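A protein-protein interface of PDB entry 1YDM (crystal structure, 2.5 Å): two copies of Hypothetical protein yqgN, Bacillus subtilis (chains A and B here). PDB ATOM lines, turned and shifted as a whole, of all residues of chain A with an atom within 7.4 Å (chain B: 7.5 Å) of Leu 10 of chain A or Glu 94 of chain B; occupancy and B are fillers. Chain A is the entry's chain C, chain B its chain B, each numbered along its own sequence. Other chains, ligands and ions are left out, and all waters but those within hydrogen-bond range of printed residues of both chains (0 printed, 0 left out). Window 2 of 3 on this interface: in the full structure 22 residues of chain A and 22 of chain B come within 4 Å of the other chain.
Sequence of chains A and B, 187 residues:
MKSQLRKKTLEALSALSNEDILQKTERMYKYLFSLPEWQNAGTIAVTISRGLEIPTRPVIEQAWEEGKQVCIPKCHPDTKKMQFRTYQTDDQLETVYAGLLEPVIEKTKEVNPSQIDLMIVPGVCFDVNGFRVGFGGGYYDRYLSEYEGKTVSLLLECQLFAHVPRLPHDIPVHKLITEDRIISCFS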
ATOM      1  N   GLN A   4       3.522 -14.267   4.786  1.00  0.00           N
ATOM      2  CA  GLN A   4       4.483 -13.141   4.953  1.00  0.00           C
ATOM      3  C   GLN A   4       3.708 -11.836   4.852  1.00  0.00           C
ATOM      4  O   GLN A   4       3.766 -10.988   5.742  1.00  0.00           O
ATOM      5  CB  GLN A   4       5.562 -13.181   3.853  1.00  0.00           C
ATOM      6  CG  GLN A   4       6.740 -12.197   4.054  1.00  0.00           C
ATOM      7  CD  GLN A   4       7.619 -12.006   2.800  1.00  0.00           C
ATOM      8  OE1 GLN A   4       8.058 -12.979   2.167  1.00  0.00           O
ATOM      9  NE2 GLN A   4       7.885 -10.745   2.451  1.00  0.00           N
ATOM     10  N   LEU A   5       2.970 -11.683   3.762  1.00  0.00           N
ATOM     11  CA  LEU A   5       2.212 -10.463   3.563  1.00  0.00           C
ATOM     12  C   LEU A   5       0.996 -10.417   4.460  1.00  0.00           C
ATOM     13  O   LEU A   5       0.698  -9.389   5.072  1.00  0.00           O
ATOM     14  CB  LEU A   5       1.776 -10.333   2.108  1.00  0.00           C
ATOM     15  CG  LEU A   5       2.902 -10.150   1.100  1.00  0.00           C
ATOM     16  CD1 LEU A   5       2.296 -10.038  -0.286  1.00  0.00           C
ATOM     17  CD2 LEU A   5       3.716  -8.907   1.429  1.00  0.00           C
ATOM     18  N   ARG A   6       0.292 -11.538   4.543  1.00  0.00           N
ATOM     19  CA  ARG A   6      -0.898 -11.586   5.370  1.00  0.00           C
ATOM     20  C   ARG A   6      -0.570 -11.176   6.812  1.00  0.00           C
ATOM     21  O   ARG A   6      -1.307 -10.405   7.436  1.00  0.00           O
ATOM     22  CB  ARG A   6      -1.497 -12.986   5.341  1.00  0.00           C
ATOM     23  CG  ARG A   6      -2.996 -12.983   5.460  1.00  0.00           C
ATOM     24  CD  ARG A   6      -3.605 -13.577   4.224  1.00  0.00           C
ATOM     25  NE  ARG A   6      -3.108 -14.932   4.022  1.00  0.00           N
ATOM     26  CZ  ARG A   6      -3.393 -15.689   2.972  1.00  0.00           C
ATOM     27  NH1 ARG A   6      -2.885 -16.903   2.893  1.00  0.00           N
ATOM     28  NH2 ARG A   6      -4.178 -15.242   2.005  1.00  0.00           N
ATOM     29  N   LYS A   7       0.552 -11.678   7.323  1.00  0.00           N
ATOM     30  CA  LYS A   7       0.986 -11.370   8.683  1.00  0.00           C
ATOM     31  C   LYS A   7       1.320  -9.891   8.838  1.00  0.00           C
ATOM     32  O   LYS A   7       0.908  -9.266   9.813  1.00  0.00           O
ATOM     33  CB  LYS A   7       2.208 -12.220   9.067  1.00  0.00           C
ATOM     34  CG  LYS A   7       2.705 -12.005  10.503  1.00  0.00           C
ATOM     35  CD  LYS A   7       4.044 -12.703  10.774  1.00  0.00           C
ATOM     36  CE  LYS A   7       3.922 -14.233  10.798  1.00  0.00           C
ATOM     37  NZ  LYS A   7       3.357 -14.754  12.080  1.00  0.00           N
ATOM     38  N   LYS A   8       2.060  -9.329   7.884  1.00  0.00           N
ATOM     39  CA  LYS A   8       2.433  -7.915   7.957  1.00  0.00           C
ATOM     40  C   LYS A   8       1.213  -7.013   8.044  1.00  0.00           C
ATOM     41  O   LYS A   8       1.183  -6.052   8.810  1.00  0.00           O
ATOM     42  CB  LYS A   8       3.284  -7.514   6.749  1.00  0.00           C
ATOM     43  CG  LYS A   8       4.734  -7.973   6.814  1.00  0.00           C
ATOM     44  CD  LYS A   8       5.457  -7.621   5.512  1.00  0.00           C
ATOM     45  CE  LYS A   8       6.825  -8.287   5.410  1.00  0.00           C
ATOM     46  NZ  LYS A   8       7.301  -8.337   3.999  1.00  0.00           N
ATOM     47  N   THR A   9       0.201  -7.347   7.257  1.00  0.00           N
ATOM     48  CA  THR A   9      -1.039  -6.591   7.234  1.00  0.00           C
ATOM     49  C   THR A   9      -1.771  -6.777   8.572  1.00  0.00           C
ATOM     50  O   THR A   9      -2.682  -6.017   8.900  1.00  0.00           O
ATOM     51  CB  THR A   9      -1.949  -7.072   6.078  1.00  0.00           C
ATOM     52  OG1 THR A   9      -1.170  -7.208   4.883  1.00  0.00           O
ATOM     53  CG2 THR A   9      -3.067  -6.081   5.824  1.00  0.00           C
ATOM     54  N   LEU A  10      -1.398  -7.798   9.338  1.00  0.00           N
ATOM     55  CA  LEU A  10      -2.047  -8.018  10.632  1.00  0.00           C
ATOM     56  C   LEU A  10      -1.430  -7.040  11.615  1.00  0.00           C
ATOM     57  O   LEU A  10      -2.140  -6.321  12.316  1.00  0.00           O
ATOM     58  CB  LEU A  10      -1.842  -9.457  11.126  1.00  0.00           C
ATOM     59  CG  LEU A  10      -2.384  -9.799  12.525  1.00  0.00           C
ATOM     60  CD1 LEU A  10      -3.893  -9.788  12.532  1.00  0.00           C
ATOM     61  CD2 LEU A  10      -1.877 -11.163  12.955  1.00  0.00           C
ATOM     62  N   GLU A  11      -0.102  -7.007  11.654  1.00  0.00           N
ATOM     63  CA  GLU A  11       0.596  -6.097  12.556  1.00  0.00           C
ATOM     64  C   GLU A  11       0.230  -4.667  12.187  1.00  0.00           C
ATOM     65  O   GLU A  11      -0.059  -3.843  13.062  1.00  0.00           O
ATOM     66  CB  GLU A  11       2.114  -6.248  12.449  1.00  0.00           C
ATOM     67  CG  GLU A  11       2.675  -7.517  13.044  1.00  0.00           C
ATOM     68  CD  GLU A  11       2.643  -8.684  12.092  1.00  0.00           C
ATOM     69  OE1 GLU A  11       3.257  -8.582  11.013  1.00  0.00           O
ATOM     70  OE2 GLU A  11       2.007  -9.711  12.419  1.00  0.00           O
ATOM     71  N   ALA A  12       0.233  -4.375  10.888  1.00  0.00           N
ATOM     72  CA  ALA A  12      -0.083  -3.025  10.434  1.00  0.00           C
ATOM     73  C   ALA A  12      -1.475  -2.583  10.879  1.00  0.00           C
ATOM     74  O   ALA A  12      -1.638  -1.507  11.461  1.00  0.00           O
ATOM     75  CB  ALA A  12       0.050  -2.937   8.925  1.00  0.00           C
ATOM     76  N   LEU A  13      -2.474  -3.416  10.614  1.00  0.00           N
ATOM     77  CA  LEU A  13      -3.848  -3.101  10.988  1.00  0.00           C
ATOM     78  C   LEU A  13      -4.064  -3.147  12.483  1.00  0.00           C
ATOM     79  O   LEU A  13      -5.044  -2.588  12.992  1.00  0.00           O
ATOM     80  CB  LEU A  13      -4.820  -4.064  10.325  1.00  0.00           C
ATOM     81  CG  LEU A  13      -4.995  -3.869   8.824  1.00  0.00           C
ATOM     82  CD1 LEU A  13      -5.724  -5.053   8.262  1.00  0.00           C
ATOM     83  CD2 LEU A  13      -5.745  -2.582   8.551  1.00  0.00           C
ATOM     84  N   SER A  14      -3.162  -3.816  13.192  1.00  0.00           N
ATOM     85  CA  SER A  14      -3.294  -3.907  14.643  1.00  0.00           C
ATOM     86  C   SER A  14      -2.689  -2.689  15.310  1.00  0.00           C
ATOM     87  O   SER A  14      -3.178  -2.229  16.330  1.00  0.00           O
ATOM     88  CB  SER A  14      -2.599  -5.163  15.169  1.00  0.00           C
ATOM     89  OG  SER A  14      -3.315  -6.337  14.828  1.00  0.00           O
ATOM     90  N   ALA A  15      -1.620  -2.177  14.712  1.00  0.00           N
ATOM     91  CA  ALA A  15      -0.898  -1.025  15.235  1.00  0.00           C
ATOM     92  C   ALA A  15      -1.746   0.234  15.266  1.00  0.00           C
ATOM     93  O   ALA A  15      -1.513   1.123  16.076  1.00  0.00           O
ATOM     94  CB  ALA A  15       0.358  -0.783  14.400  1.00  0.00           C
ATOM     95  N   LEU A  16      -2.719   0.304  14.365  1.00  0.00           N
ATOM     96  CA  LEU A  16      -3.602   1.455  14.266  1.00  0.00           C
ATOM     97  C   LEU A  16      -4.545   1.594  15.462  1.00  0.00           C
ATOM     98  O   LEU A  16      -5.087   0.611  15.979  1.00  0.00           O
ATOM     99  CB  LEU A  16      -4.419   1.373  12.968  1.00  0.00           C
ATOM    100  CG  LEU A  16      -3.654   1.612  11.662  1.00  0.00           C
ATOM    101  CD1 LEU A  16      -4.493   1.221  10.449  1.00  0.00           C
ATOM    102  CD2 LEU A  16      -3.258   3.081  11.598  1.00  0.00           C
ATOM    103  N   LEU A  52     -10.554  -7.360  11.677  1.00  0.00           N
ATOM    104  CA  LEU A  52      -9.752  -6.234  11.195  1.00  0.00           C
ATOM    105  C   LEU A  52     -10.077  -5.910   9.734  1.00  0.00           C
ATOM    106  O   LEU A  52      -9.506  -4.973   9.158  1.00  0.00           O
ATOM    107  CB  LEU A  52      -8.264  -6.555  11.334  1.00  0.00           C
ATOM    108  CG  LEU A  52      -7.792  -6.757  12.780  1.00  0.00           C
ATOM    109  CD1 LEU A  52      -6.377  -7.361  12.865  1.00  0.00           C
ATOM    110  CD2 LEU A  52      -7.840  -5.409  13.448  1.00  0.00           C
ATOM    111  N   VAL A 124      -7.228  -8.983   1.632  1.00  0.00           N
ATOM    112  CA  VAL A 124      -6.274  -8.772   2.703  1.00  0.00           C
ATOM    113  C   VAL A 124      -5.094  -7.920   2.259  1.00  0.00           C
ATOM    114  O   VAL A 124      -4.670  -7.009   2.973  1.00  0.00           O
ATOM    115  CB  VAL A 124      -5.722 -10.087   3.234  1.00  0.00           C
ATOM    116  CG1 VAL A 124      -4.814  -9.795   4.418  1.00  0.00           C
ATOM    117  CG2 VAL A 124      -6.855 -11.020   3.611  1.00  0.00           C
ATOM    118  N   CYS A 125      -4.555  -8.237   1.087  1.00  0.00           N
ATOM    119  CA  CYS A 125      -3.417  -7.502   0.541  1.00  0.00           C
ATOM    120  C   CYS A 125      -3.698  -7.076  -0.886  1.00  0.00           C
ATOM    121  O   CYS A 125      -4.368  -7.786  -1.651  1.00  0.00           O
ATOM    122  CB  CYS A 125      -2.159  -8.368   0.540  1.00  0.00           C
ATOM    123  SG  CYS A 125      -1.488  -8.753   2.146  1.00  0.00           S
ATOM    124  N   CYS A 158      -1.822   0.648   4.493  1.00  0.00           N
ATOM    125  CA  CYS A 158      -0.917  -0.404   4.965  1.00  0.00           C
ATOM    126  C   CYS A 158      -1.213  -1.799   4.394  1.00  0.00           C
ATOM    127  O   CYS A 158      -0.514  -2.763   4.704  1.00  0.00           O
ATOM    128  CB  CYS A 158      -0.903  -0.458   6.491  1.00  0.00           C
ATOM    129  SG  CYS A 158      -2.423  -1.046   7.232  1.00  0.00           S
ATOM    130  N   ARG B  57     -10.733 -18.368  20.612  1.00  0.00           N
ATOM    131  CA  ARG B  57      -9.307 -18.569  20.396  1.00  0.00           C
ATOM    132  C   ARG B  57      -8.660 -19.298  21.571  1.00  0.00           C
ATOM    133  O   ARG B  57      -8.090 -20.378  21.403  1.00  0.00           O
ATOM    134  CB  ARG B  57      -8.600 -17.227  20.160  1.00  0.00           C
ATOM    135  CG  ARG B  57      -7.068 -17.313  20.215  1.00  0.00           C
ATOM    136  CD  ARG B  57      -6.409 -16.856  18.908  1.00  0.00           C
ATOM    137  NE  ARG B  57      -6.075 -15.433  18.921  1.00  0.00           N
ATOM    138  CZ  ARG B  57      -4.845 -14.951  19.071  1.00  0.00           C
ATOM    139  NH1 ARG B  57      -3.815 -15.776  19.220  1.00  0.00           N
ATOM    140  NH2 ARG B  57      -4.649 -13.639  19.077  1.00  0.00           N
ATOM    141  N   GLU B  61      -6.643 -22.766  21.210  1.00  0.00           N
ATOM    142  CA  GLU B  61      -5.239 -22.712  21.583  1.00  0.00           C
ATOM    143  C   GLU B  61      -4.939 -23.672  22.747  1.00  0.00           C
ATOM    144  O   GLU B  61      -3.871 -24.294  22.791  1.00  0.00           O
ATOM    145  CB  GLU B  61      -4.875 -21.283  21.991  1.00  0.00           C
ATOM    146  CG  GLU B  61      -3.745 -20.654  21.187  1.00  0.00           C
ATOM    147  CD  GLU B  61      -3.844 -19.133  21.154  1.00  0.00           C
ATOM    148  OE1 GLU B  61      -3.998 -18.512  22.233  1.00  0.00           O
ATOM    149  OE2 GLU B  61      -3.761 -18.558  20.052  1.00  0.00           O
ATOM    150  N   TYR B  87      -9.606 -29.553  12.253  1.00  0.00           N
ATOM    151  CA  TYR B  87      -8.831 -28.352  12.036  1.00  0.00           C
ATOM    152  C   TYR B  87      -7.495 -28.554  12.722  1.00  0.00           C
ATOM    153  O   TYR B  87      -7.427 -28.640  13.948  1.00  0.00           O
ATOM    154  CB  TYR B  87      -9.587 -27.159  12.619  1.00  0.00           C
ATOM    155  CG  TYR B  87      -8.874 -25.830  12.589  1.00  0.00           C
ATOM    156  CD1 TYR B  87      -8.049 -25.473  11.523  1.00  0.00           C
ATOM    157  CD2 TYR B  87      -9.077 -24.895  13.612  1.00  0.00           C
ATOM    158  CE1 TYR B  87      -7.443 -24.219  11.471  1.00  0.00           C
ATOM    159  CE2 TYR B  87      -8.476 -23.633  13.576  1.00  0.00           C
ATOM    160  CZ  TYR B  87      -7.664 -23.305  12.500  1.00  0.00           C
ATOM    161  OH  TYR B  87      -7.089 -22.059  12.442  1.00  0.00           O
ATOM    162  N   ASP B  90      -2.975 -24.499  13.723  1.00  0.00           N
ATOM    163  CA  ASP B  90      -2.727 -23.408  12.799  1.00  0.00           C
ATOM    164  C   ASP B  90      -1.908 -22.283  13.414  1.00  0.00           C
ATOM    165  O   ASP B  90      -2.370 -21.587  14.321  1.00  0.00           O
ATOM    166  CB  ASP B  90      -4.068 -22.874  12.287  1.00  0.00           C
ATOM    167  CG  ASP B  90      -3.914 -21.873  11.176  1.00  0.00           C
ATOM    168  OD1 ASP B  90      -4.944 -21.493  10.577  1.00  0.00           O
ATOM    169  OD2 ASP B  90      -2.769 -21.459  10.893  1.00  0.00           O
ATOM    170  N   ASP B  91      -0.682 -22.117  12.917  1.00  0.00           N
ATOM    171  CA  ASP B  91       0.219 -21.066  13.394  1.00  0.00           C
ATOM    172  C   ASP B  91      -0.286 -19.711  12.922  1.00  0.00           C
ATOM    173  O   ASP B  91       0.288 -18.678  13.246  1.00  0.00           O
ATOM    174  CB  ASP B  91       1.644 -21.308  12.873  1.00  0.00           C
ATOM    175  CG  ASP B  91       2.593 -21.830  13.957  1.00  0.00           C
ATOM    176  OD1 ASP B  91       3.718 -22.263  13.619  1.00  0.00           O
ATOM    177  OD2 ASP B  91       2.221 -21.801  15.145  1.00  0.00           O
ATOM    178  N   GLN B  92      -1.361 -19.720  12.148  1.00  0.00           N
ATOM    179  CA  GLN B  92      -1.936 -18.476  11.659  1.00  0.00           C
ATOM    180  C   GLN B  92      -3.284 -18.286  12.335  1.00  0.00           C
ATOM    181  O   GLN B  92      -4.131 -17.524  11.877  1.00  0.00           O
ATOM    182  CB  GLN B  92      -2.107 -18.532  10.138  1.00  0.00           C
ATOM    183  CG  GLN B  92      -0.929 -19.157   9.418  1.00  0.00           C
ATOM    184  CD  GLN B  92       0.377 -18.431   9.673  1.00  0.00           C
ATOM    185  OE1 GLN B  92       1.451 -18.951   9.370  1.00  0.00           O
ATOM    186  NE2 GLN B  92       0.294 -17.222  10.223  1.00  0.00           N
ATOM    187  N   LEU B  93      -3.470 -18.998  13.435  1.00  0.00           N
ATOM    188  CA  LEU B  93      -4.710 -18.938  14.198  1.00  0.00           C
ATOM    189  C   LEU B  93      -5.117 -17.496  14.499  1.00  0.00           C
ATOM    190  O   LEU B  93      -6.287 -17.156  14.416  1.00  0.00           O
ATOM    191  CB  LEU B  93      -4.539 -19.689  15.510  1.00  0.00           C
ATOM    192  CG  LEU B  93      -5.814 -19.860  16.306  1.00  0.00           C
ATOM    193  CD1 LEU B  93      -6.618 -20.995  15.706  1.00  0.00           C
ATOM    194  CD2 LEU B  93      -5.479 -20.155  17.756  1.00  0.00           C
ATOM    195  N   GLU B  94      -4.149 -16.657  14.845  1.00  0.00           N
ATOM    196  CA  GLU B  94      -4.448 -15.276  15.161  1.00  0.00           C
ATOM    197  C   GLU B  94      -4.886 -14.514  13.910  1.00  0.00           C
ATOM    198  O   GLU B  94      -5.685 -13.575  13.980  1.00  0.00           O
ATOM    199  CB  GLU B  94      -3.222 -14.600  15.780  1.00  0.00           C
ATOM    200  CG  GLU B  94      -3.473 -13.185  16.286  1.00  0.00           C
ATOM    201  CD  GLU B  94      -2.203 -12.357  16.350  1.00  0.00           C
ATOM    202  OE1 GLU B  94      -2.297 -11.131  16.604  1.00  0.00           O
ATOM    203  OE2 GLU B  94      -1.113 -12.937  16.138  1.00  0.00           O
ATOM    204  N   THR B  95      -4.365 -14.930  12.763  1.00  0.00           N
ATOM    205  CA  THR B  95      -4.694 -14.284  11.498  1.00  0.00           C
ATOM    206  C   THR B  95      -6.137 -14.623  11.135  1.00  0.00           C
ATOM    207  O   THR B  95      -6.859 -13.802  10.560  1.00  0.00           O
ATOM    208  CB  THR B  95      -3.758 -14.766  10.365  1.00  0.00           C
ATOM    209  OG1 THR B  95      -2.398 -14.527  10.739  1.00  0.00           O
ATOM    210  CG2 THR B  95      -4.059 -14.026   9.068  1.00  0.00           C
ATOM    211  N   VAL B  96      -6.544 -15.843  11.473  1.00  0.00           N
ATOM    212  CA  VAL B  96      -7.894 -16.310  11.212  1.00  0.00           C
ATOM    213  C   VAL B  96      -8.880 -15.511  12.062  1.00  0.00           C
ATOM    214  O   VAL B  96      -9.910 -15.062  11.567  1.00  0.00           O
ATOM    215  CB  VAL B  96      -8.041 -17.806  11.571  1.00  0.00           C
ATOM    216  CG1 VAL B  96      -9.518 -18.186  11.621  1.00  0.00           C
ATOM    217  CG2 VAL B  96      -7.316 -18.670  10.543  1.00  0.00           C
ATOM    218  N   TYR B  97      -8.556 -15.338  13.343  1.00  0.00           N
ATOM    219  CA  TYR B  97      -9.421 -14.597  14.247  1.00  0.00           C
ATOM    220  C   TYR B  97      -9.480 -13.124  13.871  1.00  0.00           C
ATOM    221  O   TYR B  97     -10.436 -12.424  14.209  1.00  0.00           O
ATOM    222  CB  TYR B  97      -8.977 -14.807  15.699  1.00  0.00           C
ATOM    223  CG  TYR B  97      -9.563 -16.076  16.266  1.00  0.00           C
ATOM    224  CD1 TYR B  97     -10.723 -16.046  17.052  1.00  0.00           C
ATOM    225  CD2 TYR B  97      -9.029 -17.324  15.936  1.00  0.00           C
ATOM    226  CE1 TYR B  97     -11.333 -17.225  17.488  1.00  0.00           C
ATOM    227  CE2 TYR B  97      -9.644 -18.507  16.375  1.00  0.00           C
ATOM    228  CZ  TYR B  97     -10.793 -18.446  17.151  1.00  0.00           C
ATOM    229  OH  TYR B  97     -11.394 -19.603  17.612  1.00  0.00           O
ATOM    230  N   ALA B  98      -8.465 -12.661  13.149  1.00  0.00           N
ATOM    231  CA  ALA B  98      -8.467 -11.287  12.700  1.00  0.00           C
ATOM    232  C   ALA B  98      -9.337 -11.160  11.444  1.00  0.00           C
ATOM    233  O   ALA B  98      -9.607 -10.060  11.004  1.00  0.00           O
ATOM    234  CB  ALA B  98      -7.040 -10.808  12.426  1.00  0.00           C
ATOM    235  N   GLY B  99      -9.820 -12.279  10.901  1.00  0.00           N
ATOM    236  CA  GLY B  99     -10.646 -12.229   9.699  1.00  0.00           C
ATOM    237  C   GLY B  99      -9.834 -11.946   8.434  1.00  0.00           C
ATOM    238  O   GLY B  99     -10.383 -11.526   7.415  1.00  0.00           O
ATOM    239  N   LEU B 100      -8.523 -12.187   8.504  1.00  0.00           N
ATOM    240  CA  LEU B 100      -7.609 -11.948   7.394  1.00  0.00           C
ATOM    241  C   LEU B 100      -7.072 -13.255   6.819  1.00  0.00           C
ATOM    242  O   LEU B 100      -6.008 -13.274   6.200  1.00  0.00           O
ATOM    243  CB  LEU B 100      -6.426 -11.095   7.854  1.00  0.00           C
ATOM    244  CG  LEU B 100      -6.714  -9.904   8.752  1.00  0.00           C
ATOM    245  CD1 LEU B 100      -5.410  -9.349   9.279  1.00  0.00           C
ATOM    246  CD2 LEU B 100      -7.502  -8.845   7.995  1.00  0.00           C
ATOM    247  N   LEU B 101      -7.804 -14.340   7.033  1.00  0.00           N
ATOM    248  CA  LEU B 101      -7.414 -15.653   6.537  1.00  0.00           C
ATOM    249  C   LEU B 101      -8.401 -16.704   6.988  1.00  0.00           C
ATOM    250  O   LEU B 101      -8.485 -17.018   8.176  1.00  0.00           O
ATOM    251  CB  LEU B 101      -6.024 -16.058   7.044  1.00  0.00           C
ATOM    252  CG  LEU B 101      -5.661 -17.552   6.838  1.00  0.00           C
ATOM    253  CD1 LEU B 101      -5.740 -17.911   5.375  1.00  0.00           C
ATOM    254  CD2 LEU B 101      -4.273 -17.825   7.381  1.00  0.00           C
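The backbone carbonyl oxygen of Ala 98 of chain B sits at hydrogen-bond distance from the backbone NH of Leu 52 of chain A (2.9 Å).
The side-chain hydroxyl (OG) of Ser 14 of chain A lies within hydrogen-bond range of the backbone carbonyl oxygen (O) of Leu 10 of chain A (2.8 Å).
The backbone carbonyl oxygen (O) of Thr 95 of chain B is in hydrogen-bond range of the backbone NH (N) of Leu 100 of chain B (3.1 Å).
Among the printed residues, merely in contact across the chains: Arg 6 of chain A with Thr 95 of chain B (3.9 Å), Arg 6 of chain A with Leu 100 of chain B (3.1 Å), Arg 6 of chain A with Leu 101 of chain B (3.9 Å), Leu 10 of chain A with Glu 94 of chain B (3.6 Å), Leu 10 of chain A with Ala 98 of chain B (3.3 Å), Leu 10 of chain A with Leu 100 of chain B (3.6 Å) and Val 124 of chain A with Leu 100 of chain B (3.5 Å).
Of chain B, only Glu 94 (3.6 Å), Ala 98 (3.3 Å) and Leu 100 (3.6 Å) come within 4 Å of Leu 10 of chain A.
Of chain A, only Leu 10 (3.6 Å) comes within 4 Å of Glu 94 of chain B.
Of the printed residues of chain A, Ala 98 of chain B touches Leu 10 and Leu 52.
Printed residues of chain B within 4 Å of Val 124 of chain A: Leu 100 (3.5 Å).
The nearest residue of chain B that does not touch Leu 10 of chain A is Thr 95 of chain B (4.1 Å).
The nearest residue of chain A that does not touch Glu 94 of chain B is Ser 14 of chain A (5.2 Å).
The nearest printed residue of chain B that does not touch Val 124 of chain A is Leu 101 of chain B (4.9 Å).
Of the 15 printed residues of chain B, 5 touch a printed residue of chain A.
Of the 17 printed residues of chain A, 4 touch a printed residue of chain B.
Hydrophobic or aromatic side chains of chain A that line the printed part of chain B: Leu 10, Leu 52 and Val 124.
No position is printed for both chains.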
